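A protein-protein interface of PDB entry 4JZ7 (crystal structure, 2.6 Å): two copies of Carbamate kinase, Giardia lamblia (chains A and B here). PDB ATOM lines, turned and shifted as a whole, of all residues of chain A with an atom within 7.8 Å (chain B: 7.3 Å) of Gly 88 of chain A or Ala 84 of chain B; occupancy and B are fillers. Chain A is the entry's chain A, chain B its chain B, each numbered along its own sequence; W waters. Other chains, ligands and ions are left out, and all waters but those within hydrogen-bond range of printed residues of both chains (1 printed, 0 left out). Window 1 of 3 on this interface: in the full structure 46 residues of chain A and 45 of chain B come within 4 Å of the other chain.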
ATOM      1  N   ILE A  63      10.651   7.134   3.239  1.00  0.00           N
ATOM      2  CA  ILE A  63      12.069   7.428   3.321  1.00  0.00           C
ATOM      3  C   ILE A  63      12.450   7.875   4.747  1.00  0.00           C
ATOM      4  O   ILE A  63      13.411   7.357   5.316  1.00  0.00           O
ATOM      5  CB  ILE A  63      12.505   8.494   2.250  1.00  0.00           C
ATOM      6  CG1 ILE A  63      12.574   7.861   0.858  1.00  0.00           C
ATOM      7  CG2 ILE A  63      13.863   9.095   2.584  1.00  0.00           C
ATOM      8  CD1 ILE A  63      12.813   8.837  -0.264  1.00  0.00           C
ATOM      9  N   CYS A  82      15.650  13.919   2.781  1.00  0.00           N
ATOM     10  CA  CYS A  82      14.683  12.862   2.464  1.00  0.00           C
ATOM     11  C   CYS A  82      13.769  13.323   1.365  1.00  0.00           C
ATOM     12  O   CYS A  82      13.463  12.557   0.430  1.00  0.00           O
ATOM     13  CB  CYS A  82      13.820  12.531   3.674  1.00  0.00           C
ATOM     14  SG  CYS A  82      14.699  11.722   5.015  1.00  0.00           S
ATOM     15  N   GLY A  83      13.323  14.572   1.488  1.00  0.00           N
ATOM     16  CA  GLY A  83      12.486  15.159   0.454  1.00  0.00           C
ATOM     17  C   GLY A  83      13.156  14.985  -0.899  1.00  0.00           C
ATOM     18  O   GLY A  83      12.522  14.578  -1.880  1.00  0.00           O
ATOM     19  N   ALA A  84      14.459  15.278  -0.922  1.00  0.00           N
ATOM     20  CA  ALA A  84      15.240  15.236  -2.137  1.00  0.00           C
ATOM     21  C   ALA A  84      15.273  13.833  -2.758  1.00  0.00           C
ATOM     22  O   ALA A  84      15.072  13.708  -3.964  1.00  0.00           O
ATOM     23  CB  ALA A  84      16.627  15.745  -1.885  1.00  0.00           C
ATOM     24  N   MET A  85      15.547  12.793  -1.966  1.00  0.00           N
ATOM     25  CA  MET A  85      15.608  11.445  -2.532  1.00  0.00           C
ATOM     26  C   MET A  85      14.243  11.064  -3.106  1.00  0.00           C
ATOM     27  O   MET A  85      14.139  10.307  -4.078  1.00  0.00           O
ATOM     28  CB  MET A  85      16.039  10.408  -1.494  1.00  0.00           C
ATOM     29  CG  MET A  85      17.056  10.882  -0.506  1.00  0.00           C
ATOM     30  SD  MET A  85      17.559   9.614   0.698  1.00  0.00           S
ATOM     31  CE  MET A  85      18.213  10.617   2.016  1.00  0.00           C
ATOM     32  N   SER A  86      13.185  11.577  -2.479  1.00  0.00           N
ATOM     33  CA  SER A  86      11.829  11.296  -2.927  1.00  0.00           C
ATOM     34  C   SER A  86      11.564  11.940  -4.285  1.00  0.00           C
ATOM     35  O   SER A  86      10.720  11.469  -5.043  1.00  0.00           O
ATOM     36  CB  SER A  86      10.809  11.762  -1.883  1.00  0.00           C
ATOM     37  OG  SER A  86      10.472  13.123  -2.055  1.00  0.00           O
ATOM     38  N   GLN A  87      12.228  13.047  -4.587  1.00  0.00           N
ATOM     39  CA  GLN A  87      12.021  13.642  -5.906  1.00  0.00           C
ATOM     40  C   GLN A  87      12.662  12.766  -6.999  1.00  0.00           C
ATOM     41  O   GLN A  87      12.072  12.545  -8.065  1.00  0.00           O
ATOM     42  CB  GLN A  87      12.515  15.106  -5.943  1.00  0.00           C
ATOM     43  CG  GLN A  87      11.582  16.098  -5.214  1.00  0.00           C
ATOM     44  CD  GLN A  87      12.090  17.540  -5.287  1.00  0.00           C
ATOM     45  OE1 GLN A  87      13.087  17.816  -5.964  1.00  0.00           O
ATOM     46  NE2 GLN A  87      11.415  18.459  -4.587  1.00  0.00           N
ATOM     47  N   GLY A  88      13.874  12.289  -6.745  1.00  0.00           N
ATOM     48  CA  GLY A  88      14.496  11.345  -7.647  1.00  0.00           C
ATOM     49  C   GLY A  88      13.605  10.126  -7.852  1.00  0.00           C
ATOM     50  O   GLY A  88      13.410   9.651  -8.990  1.00  0.00           O
ATOM     51  N   PHE A  89      13.083   9.605  -6.742  1.00  0.00           N
ATOM     52  CA  PHE A  89      12.209   8.452  -6.806  1.00  0.00           C
ATOM     53  C   PHE A  89      11.027   8.775  -7.688  1.00  0.00           C
ATOM     54  O   PHE A  89      10.819   8.153  -8.734  1.00  0.00           O
ATOM     55  CB  PHE A  89      11.705   8.061  -5.413  1.00  0.00           C
ATOM     56  CG  PHE A  89      10.871   6.804  -5.403  1.00  0.00           C
ATOM     57  CD1 PHE A  89      11.021   5.838  -6.405  1.00  0.00           C
ATOM     58  CD2 PHE A  89       9.924   6.588  -4.413  1.00  0.00           C
ATOM     59  CE1 PHE A  89      10.252   4.663  -6.421  1.00  0.00           C
ATOM     60  CE2 PHE A  89       9.151   5.410  -4.421  1.00  0.00           C
ATOM     61  CZ  PHE A  89       9.320   4.449  -5.431  1.00  0.00           C
ATOM     62  N   ILE A  90      10.243   9.743  -7.235  1.00  0.00           N
ATOM     63  CA  ILE A  90       8.996  10.096  -7.916  1.00  0.00           C
ATOM     64  C   ILE A  90       9.272  10.533  -9.359  1.00  0.00           C
ATOM     65  O   ILE A  90       8.704   9.967 -10.304  1.00  0.00           O
ATOM     66  CB  ILE A  90       8.213  11.171  -7.091  1.00  0.00           C
ATOM     67  CG1 ILE A  90       7.667  10.540  -5.801  1.00  0.00           C
ATOM     68  CG2 ILE A  90       7.088  11.778  -7.889  1.00  0.00           C
ATOM     69  CD1 ILE A  90       7.367  11.547  -4.707  1.00  0.00           C
ATOM     70  N   GLY A  91      10.136  11.541  -9.518  1.00  0.00           N
ATOM     71  CA  GLY A  91      10.613  11.963 -10.822  1.00  0.00           C
ATOM     72  C   GLY A  91      10.975  10.811 -11.744  1.00  0.00           C
ATOM     73  O   GLY A  91      10.466  10.696 -12.846  1.00  0.00           O
ATOM     74  N   TYR A  92      11.896   9.969 -11.300  1.00  0.00           N
ATOM     75  CA  TYR A  92      12.265   8.769 -12.056  1.00  0.00           C
ATOM     76  C   TYR A  92      11.025   8.087 -12.649  1.00  0.00           C
ATOM     77  O   TYR A  92      10.886   8.000 -13.869  1.00  0.00           O
ATOM     78  CB  TYR A  92      13.046   7.809 -11.146  1.00  0.00           C
ATOM     79  CG  TYR A  92      13.197   6.394 -11.659  1.00  0.00           C
ATOM     80  CD1 TYR A  92      13.563   6.127 -12.977  1.00  0.00           C
ATOM     81  CD2 TYR A  92      13.004   5.321 -10.810  1.00  0.00           C
ATOM     82  CE1 TYR A  92      13.701   4.838 -13.427  1.00  0.00           C
ATOM     83  CE2 TYR A  92      13.150   4.036 -11.246  1.00  0.00           C
ATOM     84  CZ  TYR A  92      13.496   3.790 -12.551  1.00  0.00           C
ATOM     85  OH  TYR A  92      13.625   2.477 -12.951  1.00  0.00           O
ATOM     86  N   MET A  93      10.138   7.601 -11.777  1.00  0.00           N
ATOM     87  CA  MET A  93       8.882   6.963 -12.175  1.00  0.00           C
ATOM     88  C   MET A  93       8.056   7.721 -13.221  1.00  0.00           C
ATOM     89  O   MET A  93       7.661   7.164 -14.263  1.00  0.00           O
ATOM     90  CB  MET A  93       8.033   6.685 -10.935  1.00  0.00           C
ATOM     91  CG  MET A  93       8.492   5.466 -10.157  1.00  0.00           C
ATOM     92  SD  MET A  93       7.267   4.865  -8.971  1.00  0.00           S
ATOM     93  CE  MET A  93       7.151   6.302  -7.877  1.00  0.00           C
ATOM     94  N   MET A  94       7.758   8.983 -12.940  1.00  0.00           N
ATOM     95  CA  MET A  94       6.973   9.762 -13.883  1.00  0.00           C
ATOM     96  C   MET A  94       7.716   9.947 -15.206  1.00  0.00           C
ATOM     97  O   MET A  94       7.104   9.818 -16.270  1.00  0.00           O
ATOM     98  CB  MET A  94       6.566  11.095 -13.275  1.00  0.00           C
ATOM     99  CG  MET A  94       5.451  10.933 -12.273  1.00  0.00           C
ATOM    100  SD  MET A  94       5.127  12.439 -11.336  1.00  0.00           S
ATOM    101  CE  MET A  94       4.146  11.747  -9.987  1.00  0.00           C
ATOM    102  N   SER A  95       9.020  10.238 -15.123  1.00  0.00           N
ATOM    103  CA  SER A  95       9.891  10.292 -16.285  1.00  0.00           C
ATOM    104  C   SER A  95       9.737   9.034 -17.108  1.00  0.00           C
ATOM    105  O   SER A  95       9.478   9.091 -18.321  1.00  0.00           O
ATOM    106  CB  SER A  95      11.350  10.329 -15.864  1.00  0.00           C
ATOM    107  OG  SER A  95      11.736  11.604 -15.425  1.00  0.00           O
ATOM    108  N   THR A 113      12.953  15.312 -15.573  1.00  0.00           N
ATOM    109  CA  THR A 113      12.655  15.700 -14.204  1.00  0.00           C
ATOM    110  C   THR A 113      13.745  16.601 -13.615  1.00  0.00           C
ATOM    111  O   THR A 113      14.943  16.323 -13.708  1.00  0.00           O
ATOM    112  CB  THR A 113      12.400  14.486 -13.303  1.00  0.00           C
ATOM    113  OG1 THR A 113      11.318  13.745 -13.851  1.00  0.00           O
ATOM    114  CG2 THR A 113      11.996  14.929 -11.889  1.00  0.00           C
ATOM    115  N   CYS A 114      13.313  17.697 -13.020  1.00  0.00           N
ATOM    116  CA  CYS A 114      14.242  18.617 -12.395  1.00  0.00           C
ATOM    117  C   CYS A 114      14.091  18.523 -10.883  1.00  0.00           C
ATOM    118  O   CYS A 114      12.990  18.683 -10.350  1.00  0.00           O
ATOM    119  CB  CYS A 114      13.981  20.037 -12.869  1.00  0.00           C
ATOM    120  SG  CYS A 114      13.911  20.204 -14.693  1.00  0.00           S
ATOM    121  N   VAL A 115      15.188  18.228 -10.188  1.00  0.00           N
ATOM    122  CA  VAL A 115      15.214  18.467  -8.756  1.00  0.00           C
ATOM    123  C   VAL A 115      14.767  19.914  -8.539  1.00  0.00           C
ATOM    124  O   VAL A 115      15.165  20.817  -9.287  1.00  0.00           O
ATOM    125  CB  VAL A 115      16.623  18.237  -8.177  1.00  0.00           C
ATOM    126  CG1 VAL A 115      16.725  18.820  -6.783  1.00  0.00           C
ATOM    127  CG2 VAL A 115      16.922  16.738  -8.161  1.00  0.00           C
ATOM    128  N   ASN A 195       7.979  18.015  -7.311  1.00  0.00           N
ATOM    129  CA  ASN A 195       7.317  16.862  -6.719  1.00  0.00           C
ATOM    130  C   ASN A 195       7.379  16.873  -5.185  1.00  0.00           C
ATOM    131  O   ASN A 195       8.440  16.665  -4.583  1.00  0.00           O
ATOM    132  CB  ASN A 195       7.886  15.561  -7.269  1.00  0.00           C
ATOM    133  CG  ASN A 195       7.797  15.481  -8.760  1.00  0.00           C
ATOM    134  OD1 ASN A 195       8.821  15.568  -9.446  1.00  0.00           O
ATOM    135  ND2 ASN A 195       6.573  15.318  -9.285  1.00  0.00           N
ATOM    136  N   ILE A 199      11.906  21.025  -2.500  1.00  0.00           N
ATOM    137  CA  ILE A 199      12.752  20.926  -1.320  1.00  0.00           C
ATOM    138  C   ILE A 199      12.790  22.285  -0.603  1.00  0.00           C
ATOM    139  O   ILE A 199      13.223  23.268  -1.172  1.00  0.00           O
ATOM    140  CB  ILE A 199      14.143  20.445  -1.702  1.00  0.00           C
ATOM    141  CG1 ILE A 199      14.036  19.009  -2.211  1.00  0.00           C
ATOM    142  CG2 ILE A 199      15.083  20.547  -0.513  1.00  0.00           C
ATOM    143  CD1 ILE A 199      15.177  18.567  -3.091  1.00  0.00           C
ATOM    144  N   ASN B  56      28.213   7.621  -7.398  1.00  0.00           N
ATOM    145  CA  ASN B  56      27.241   7.544  -6.311  1.00  0.00           C
ATOM    146  C   ASN B  56      27.478   6.412  -5.314  1.00  0.00           C
ATOM    147  O   ASN B  56      26.769   6.312  -4.304  1.00  0.00           O
ATOM    148  CB  ASN B  56      25.806   7.489  -6.871  1.00  0.00           C
ATOM    149  CG  ASN B  56      25.576   6.279  -7.758  1.00  0.00           C
ATOM    150  OD1 ASN B  56      26.525   5.595  -8.139  1.00  0.00           O
ATOM    151  ND2 ASN B  56      24.314   6.005  -8.086  1.00  0.00           N
ATOM    152  N   VAL B  60      24.465   5.578  -2.851  1.00  0.00           N
ATOM    153  CA  VAL B  60      23.520   4.537  -3.234  1.00  0.00           C
ATOM    154  C   VAL B  60      23.691   3.385  -2.238  1.00  0.00           C
ATOM    155  O   VAL B  60      22.704   2.812  -1.760  1.00  0.00           O
ATOM    156  CB  VAL B  60      23.766   4.097  -4.717  1.00  0.00           C
ATOM    157  CG1 VAL B  60      24.802   2.982  -4.806  1.00  0.00           C
ATOM    158  CG2 VAL B  60      22.482   3.699  -5.402  1.00  0.00           C
ATOM    159  N   ILE B  63      22.037   4.204   0.865  1.00  0.00           N
ATOM    160  CA  ILE B  63      20.618   4.044   0.598  1.00  0.00           C
ATOM    161  C   ILE B  63      20.235   2.566   0.518  1.00  0.00           C
ATOM    162  O   ILE B  63      19.324   2.147   1.231  1.00  0.00           O
ATOM    163  CB  ILE B  63      20.175   4.804  -0.674  1.00  0.00           C
ATOM    164  CG1 ILE B  63      19.981   6.286  -0.339  1.00  0.00           C
ATOM    165  CG2 ILE B  63      18.854   4.229  -1.219  1.00  0.00           C
ATOM    166  CD1 ILE B  63      20.242   7.208  -1.507  1.00  0.00           C
ATOM    167  N   PRO B  78      14.114  -1.491  -4.687  1.00  0.00           N
ATOM    168  CA  PRO B  78      15.173  -2.187  -5.440  1.00  0.00           C
ATOM    169  C   PRO B  78      16.412  -1.329  -5.697  1.00  0.00           C
ATOM    170  O   PRO B  78      16.509  -0.195  -5.219  1.00  0.00           O
ATOM    171  CB  PRO B  78      14.487  -2.559  -6.755  1.00  0.00           C
ATOM    172  CG  PRO B  78      13.371  -1.556  -6.908  1.00  0.00           C
ATOM    173  CD  PRO B  78      12.952  -1.134  -5.521  1.00  0.00           C
ATOM    174  N   LEU B  79      17.364  -1.870  -6.448  1.00  0.00           N
ATOM    175  CA  LEU B  79      18.635  -1.177  -6.635  1.00  0.00           C
ATOM    176  C   LEU B  79      18.462   0.101  -7.458  1.00  0.00           C
ATOM    177  O   LEU B  79      18.956   1.158  -7.077  1.00  0.00           O
ATOM    178  CB  LEU B  79      19.669  -2.116  -7.282  1.00  0.00           C
ATOM    179  CG  LEU B  79      21.102  -1.595  -7.388  1.00  0.00           C
ATOM    180  CD1 LEU B  79      21.545  -1.005  -6.059  1.00  0.00           C
ATOM    181  CD2 LEU B  79      22.061  -2.684  -7.850  1.00  0.00           C
ATOM    182  N   HIS B  80      17.778  -0.007  -8.591  1.00  0.00           N
ATOM    183  CA  HIS B  80      17.667   1.127  -9.488  1.00  0.00           C
ATOM    184  C   HIS B  80      16.850   2.268  -8.845  1.00  0.00           C
ATOM    185  O   HIS B  80      17.150   3.452  -9.034  1.00  0.00           O
ATOM    186  CB  HIS B  80      17.168   0.703 -10.882  1.00  0.00           C
ATOM    187  CG  HIS B  80      15.797   0.104 -10.896  1.00  0.00           C
ATOM    188  ND1 HIS B  80      14.648   0.868 -10.914  1.00  0.00           N
ATOM    189  CD2 HIS B  80      15.392  -1.189 -10.905  1.00  0.00           C
ATOM    190  CE1 HIS B  80      13.592   0.069 -10.915  1.00  0.00           C
ATOM    191  NE2 HIS B  80      14.017  -1.182 -10.905  1.00  0.00           N
ATOM    192  N   VAL B  81      15.847   1.931  -8.042  1.00  0.00           N
ATOM    193  CA  VAL B  81      15.132   2.976  -7.326  1.00  0.00           C
ATOM    194  C   VAL B  81      16.016   3.633  -6.244  1.00  0.00           C
ATOM    195  O   VAL B  81      15.975   4.852  -6.026  1.00  0.00           O
ATOM    196  CB  VAL B  81      13.815   2.450  -6.725  1.00  0.00           C
ATOM    197  CG1 VAL B  81      13.297   3.388  -5.641  1.00  0.00           C
ATOM    198  CG2 VAL B  81      12.794   2.275  -7.805  1.00  0.00           C
ATOM    199  N   CYS B  82      16.833   2.840  -5.565  1.00  0.00           N
ATOM    200  CA  CYS B  82      17.858   3.428  -4.697  1.00  0.00           C
ATOM    201  C   CYS B  82      18.722   4.424  -5.482  1.00  0.00           C
ATOM    202  O   CYS B  82      19.023   5.527  -4.995  1.00  0.00           O
ATOM    203  CB  CYS B  82      18.710   2.339  -4.035  1.00  0.00           C
ATOM    204  SG  CYS B  82      17.786   1.388  -2.771  1.00  0.00           S
ATOM    205  N   GLY B  83      19.136   4.015  -6.686  1.00  0.00           N
ATOM    206  CA  GLY B  83      19.858   4.883  -7.605  1.00  0.00           C
ATOM    207  C   GLY B  83      19.155   6.205  -7.858  1.00  0.00           C
ATOM    208  O   GLY B  83      19.777   7.268  -7.762  1.00  0.00           O
ATOM    209  N   ALA B  84      17.859   6.123  -8.181  1.00  0.00           N
ATOM    210  CA  ALA B  84      17.026   7.307  -8.399  1.00  0.00           C
ATOM    211  C   ALA B  84      16.931   8.175  -7.138  1.00  0.00           C
ATOM    212  O   ALA B  84      16.763   9.382  -7.221  1.00  0.00           O
ATOM    213  CB  ALA B  84      15.668   6.919  -8.851  1.00  0.00           C
ATOM    214  N   MET B  85      17.058   7.557  -5.971  1.00  0.00           N
ATOM    215  CA  MET B  85      17.059   8.301  -4.724  1.00  0.00           C
ATOM    216  C   MET B  85      18.422   8.989  -4.475  1.00  0.00           C
ATOM    217  O   MET B  85      18.491  10.115  -3.956  1.00  0.00           O
ATOM    218  CB  MET B  85      16.680   7.386  -3.557  1.00  0.00           C
ATOM    219  CG  MET B  85      15.225   6.979  -3.531  1.00  0.00           C
ATOM    220  SD  MET B  85      14.784   6.051  -2.024  1.00  0.00           S
ATOM    221  CE  MET B  85      13.004   5.855  -2.198  1.00  0.00           C
ATOM    222  N   SER B  86      19.504   8.319  -4.852  1.00  0.00           N
ATOM    223  CA  SER B  86      20.823   8.885  -4.665  1.00  0.00           C
ATOM    224  C   SER B  86      20.964  10.092  -5.582  1.00  0.00           C
ATOM    225  O   SER B  86      21.647  11.076  -5.257  1.00  0.00           O
ATOM    226  CB  SER B  86      21.899   7.842  -4.988  1.00  0.00           C
ATOM    227  OG  SER B  86      22.037   7.673  -6.385  1.00  0.00           O
ATOM    228  N   GLN B  87      20.347   9.987  -6.754  1.00  0.00           N
ATOM    229  CA  GLN B  87      20.367  11.062  -7.740  1.00  0.00           C
ATOM    230  C   GLN B  87      19.668  12.325  -7.236  1.00  0.00           C
ATOM    231  O   GLN B  87      20.181  13.423  -7.410  1.00  0.00           O
ATOM    232  CB  GLN B  87      19.755  10.606  -9.075  1.00  0.00           C
ATOM    233  CG  GLN B  87      20.757  10.012 -10.054  1.00  0.00           C
ATOM    234  CD  GLN B  87      20.177   9.813 -11.444  1.00  0.00           C
ATOM    235  OE1 GLN B  87      19.278  10.565 -11.876  1.00  0.00           O
ATOM    236  NE2 GLN B  87      20.679   8.797 -12.158  1.00  0.00           N
ATOM    237  N   GLY B  88      18.474  12.174  -6.667  1.00  0.00           N
ATOM    238  CA  GLY B  88      17.765  13.329  -6.151  1.00  0.00           C
ATOM    239  C   GLY B  88      18.634  14.030  -5.111  1.00  0.00           C
ATOM    240  O   GLY B  88      18.899  15.232  -5.168  1.00  0.00           O
ATOM    241  N   PHE B  89      19.079  13.241  -4.143  1.00  0.00           N
ATOM    242  CA  PHE B  89      19.867  13.699  -3.005  1.00  0.00           C
ATOM    243  C   PHE B  89      21.156  14.400  -3.427  1.00  0.00           C
ATOM    244  O   PHE B  89      21.418  15.541  -2.993  1.00  0.00           O
ATOM    245  CB  PHE B  89      20.248  12.453  -2.201  1.00  0.00           C
ATOM    246  CG  PHE B  89      21.298  12.682  -1.155  1.00  0.00           C
ATOM    247  CD1 PHE B  89      21.492  13.939  -0.602  1.00  0.00           C
ATOM    248  CD2 PHE B  89      22.092  11.628  -0.715  1.00  0.00           C
ATOM    249  CE1 PHE B  89      22.452  14.149   0.383  1.00  0.00           C
ATOM    250  CE2 PHE B  89      23.041  11.832   0.269  1.00  0.00           C
ATOM    251  CZ  PHE B  89      23.218  13.100   0.819  1.00  0.00           C
ATOM    252  N   VAL B 115      17.016  14.285 -13.342  1.00  0.00           N
ATOM    253  CA  VAL B 115      16.954  12.838 -13.157  1.00  0.00           C
ATOM    254  C   VAL B 115      17.272  12.125 -14.480  1.00  0.00           C
ATOM    255  O   VAL B 115      16.724  12.441 -15.535  1.00  0.00           O
ATOM    256  CB  VAL B 115      15.588  12.374 -12.621  1.00  0.00           C
ATOM    257  CG1 VAL B 115      15.475  10.839 -12.713  1.00  0.00           C
ATOM    258  CG2 VAL B 115      15.391  12.840 -11.182  1.00  0.00           C
ATOM    259  N   THR B 116      18.169  11.150 -14.417  1.00  0.00           N
ATOM    260  CA  THR B 116      18.689  10.556 -15.632  1.00  0.00           C
ATOM    261  C   THR B 116      18.620   9.051 -15.689  1.00  0.00           C
ATOM    262  O   THR B 116      18.931   8.380 -14.720  1.00  0.00           O
ATOM    263  CB  THR B 116      20.160  10.928 -15.813  1.00  0.00           C
ATOM    264  OG1 THR B 116      20.290  12.360 -15.754  1.00  0.00           O
ATOM    265  CG2 THR B 116      20.674  10.365 -17.152  1.00  0.00           C
ATOM    266  N   ASN B 195      24.202  11.631 -12.546  1.00  0.00           N
ATOM    267  CA  ASN B 195      24.774  11.401 -11.231  1.00  0.00           C
ATOM    268  C   ASN B 195      24.805   9.910 -10.918  1.00  0.00           C
ATOM    269  O   ASN B 195      23.769   9.245 -10.945  1.00  0.00           O
ATOM    270  CB  ASN B 195      23.949  12.114 -10.167  1.00  0.00           C
ATOM    271  CG  ASN B 195      24.085  13.603 -10.237  1.00  0.00           C
ATOM    272  OD1 ASN B 195      23.091  14.309 -10.445  1.00  0.00           O
ATOM    273  ND2 ASN B 195      25.323  14.109 -10.052  1.00  0.00           N
ATOM    274  N   GLY B 198      23.717   7.366 -13.969  1.00  0.00           N
ATOM    275  CA  GLY B 198      22.359   7.159 -14.449  1.00  0.00           C
ATOM    276  C   GLY B 198      21.723   5.918 -13.846  1.00  0.00           C
ATOM    277  O   GLY B 198      22.416   4.950 -13.531  1.00  0.00           O
ATOM    278  N   ILE B 199      20.403   5.973 -13.660  1.00  0.00           N
ATOM    279  CA  ILE B 199      19.587   4.824 -13.273  1.00  0.00           C
ATOM    280  C   ILE B 199      19.573   3.731 -14.355  1.00  0.00           C
ATOM    281  O   ILE B 199      19.051   3.919 -15.453  1.00  0.00           O
ATOM    282  CB  ILE B 199      18.150   5.285 -13.104  1.00  0.00           C
ATOM    283  CG1 ILE B 199      18.026   6.179 -11.871  1.00  0.00           C
ATOM    284  CG2 ILE B 199      17.208   4.094 -13.058  1.00  0.00           C
ATOM    285  CD1 ILE B 199      17.108   7.364 -12.088  1.00  0.00           C
ATOM    286  N   PRO B 200      20.137   2.560 -14.043  1.00  0.00           N
ATOM    287  CA  PRO B 200      20.247   1.519 -15.083  1.00  0.00           C
ATOM    288  C   PRO B 200      18.867   1.119 -15.578  1.00  0.00           C
ATOM    289  O   PRO B 200      17.964   0.895 -14.772  1.00  0.00           O
ATOM    290  CB  PRO B 200      20.899   0.342 -14.352  1.00  0.00           C
ATOM    291  CG  PRO B 200      21.364   0.897 -12.988  1.00  0.00           C
ATOM    292  CD  PRO B 200      20.462   2.058 -12.696  1.00  0.00           C
HETATM  293  O   HOH W   1      14.269  12.052 -16.296  1.00  0.00           O
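OH of Tyr 92 of chain A lies within hydrogen-bond range of ND1 of His 80 of chain B (2.8 Å). O of Thr 113 of chain A is in hydrogen-bond range of N of Val 115 of chain B (2.9 Å).
The side-chain hydroxyl (OG1) of Thr 113 of chain A is in hydrogen-bond range of the backbone carbonyl oxygen (O) of Gly 91 of chain A. The side-chain hydroxyl (OG1) of Thr 113 of chain A sits at hydrogen-bond distance from the side-chain hydroxyl (OG) of Ser 95 of chain A. The backbone NH of Ile 199 of chain B lies close to the side-chain amide nitrogen of Gln 87 of chain B. O of Thr 116 of chain B is in hydrogen-bond range of N of Ile 199 of chain B (3.0 Å).
Met 85 of chain B touches Ile 63 of chain A. Gly 88 of chain B touches Ala 84 of chain A (CA to O, 3.5 Å). CA of Phe 89 of chain B touches CB of Ala 84 of chain A, at 3.99 Å. Ala 84 of chain B touches Gly 88 of chain A (O to CA, 3.0 Å). Gly 88 of chain A touches Val 115 of chain B. Phe 89 of chain A touches Val 81 of chain B (CE1 to CG1, 3.4 Å). Phe 89 of chain A touches Ala 84 of chain B (N to O, 3.7 Å). Tyr 92 of chain A touches Val 81 of chain B (CE2 to CG2, 3.9 Å). Tyr 92 of chain A touches Ile 199 of chain B. Val 115 of chain A touches Gly 88 of chain B (CG2 to O, 3.9 Å).
Gly 88 of chain A touches just these residues of chain B: Ala 84 and Val 115. Ala 84 of chain B touches just these residues of chain A: Gly 88 (3.0 Å), Phe 89 (3.7 Å) and Tyr 92 (3.6 Å). Of the printed residues of chain B, Ala 84 of chain A touches Gly 88 and Phe 89. Of the printed residues of chain A, Val 115 of chain B touches Gly 88 (3.9 Å), Tyr 92 (3.9 Å) and Thr 113 (2.9 Å). Printed residues of chain B within 4 Å of Met 85 of chain A: Met 85 and Phe 89. The nearest printed residue of chain B that does not touch Ala 84 of chain A is Met 85 of chain B (5.0 Å).
Of the 20 printed residues of chain A, 8 touch a printed residue of chain B. Along chain A the printed residues that touch a printed residue of chain B span positions 63 to 115. Hydrophobic or aromatic side chains of chain B within 4 Å of the printed part of chain A: His 80, Val 81, Ala 84, Met 85, Phe 89, Val 115 and Ile 199. Among the printed residues, no Asp or Glu carboxylate lies within 4 Å of a Lys or Arg side-chain nitrogen of the other chain.
Ala 84 of chain A touches Gly 88 of chain B, and with the chains exchanged Gly 88 of chain A touches Ala 84 of chain B. Ala 84 of chain A touches Phe 89 of chain B, and with the chains exchanged Phe 89 of chain A touches Ala 84 of chain B. Met 85 of chain A touches Phe 89 of chain B, and with the chains exchanged Phe 89 of chain A touches Met 85 of chain B. Gly 88 of chain A touches Val 115 of chain B, and with the chains exchanged Val 115 of chain A touches Gly 88 of chain B.
Water W1 lies within hydrogen-bond range of O of Val 115 of chain B and OG of Ser 95 of chain A.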
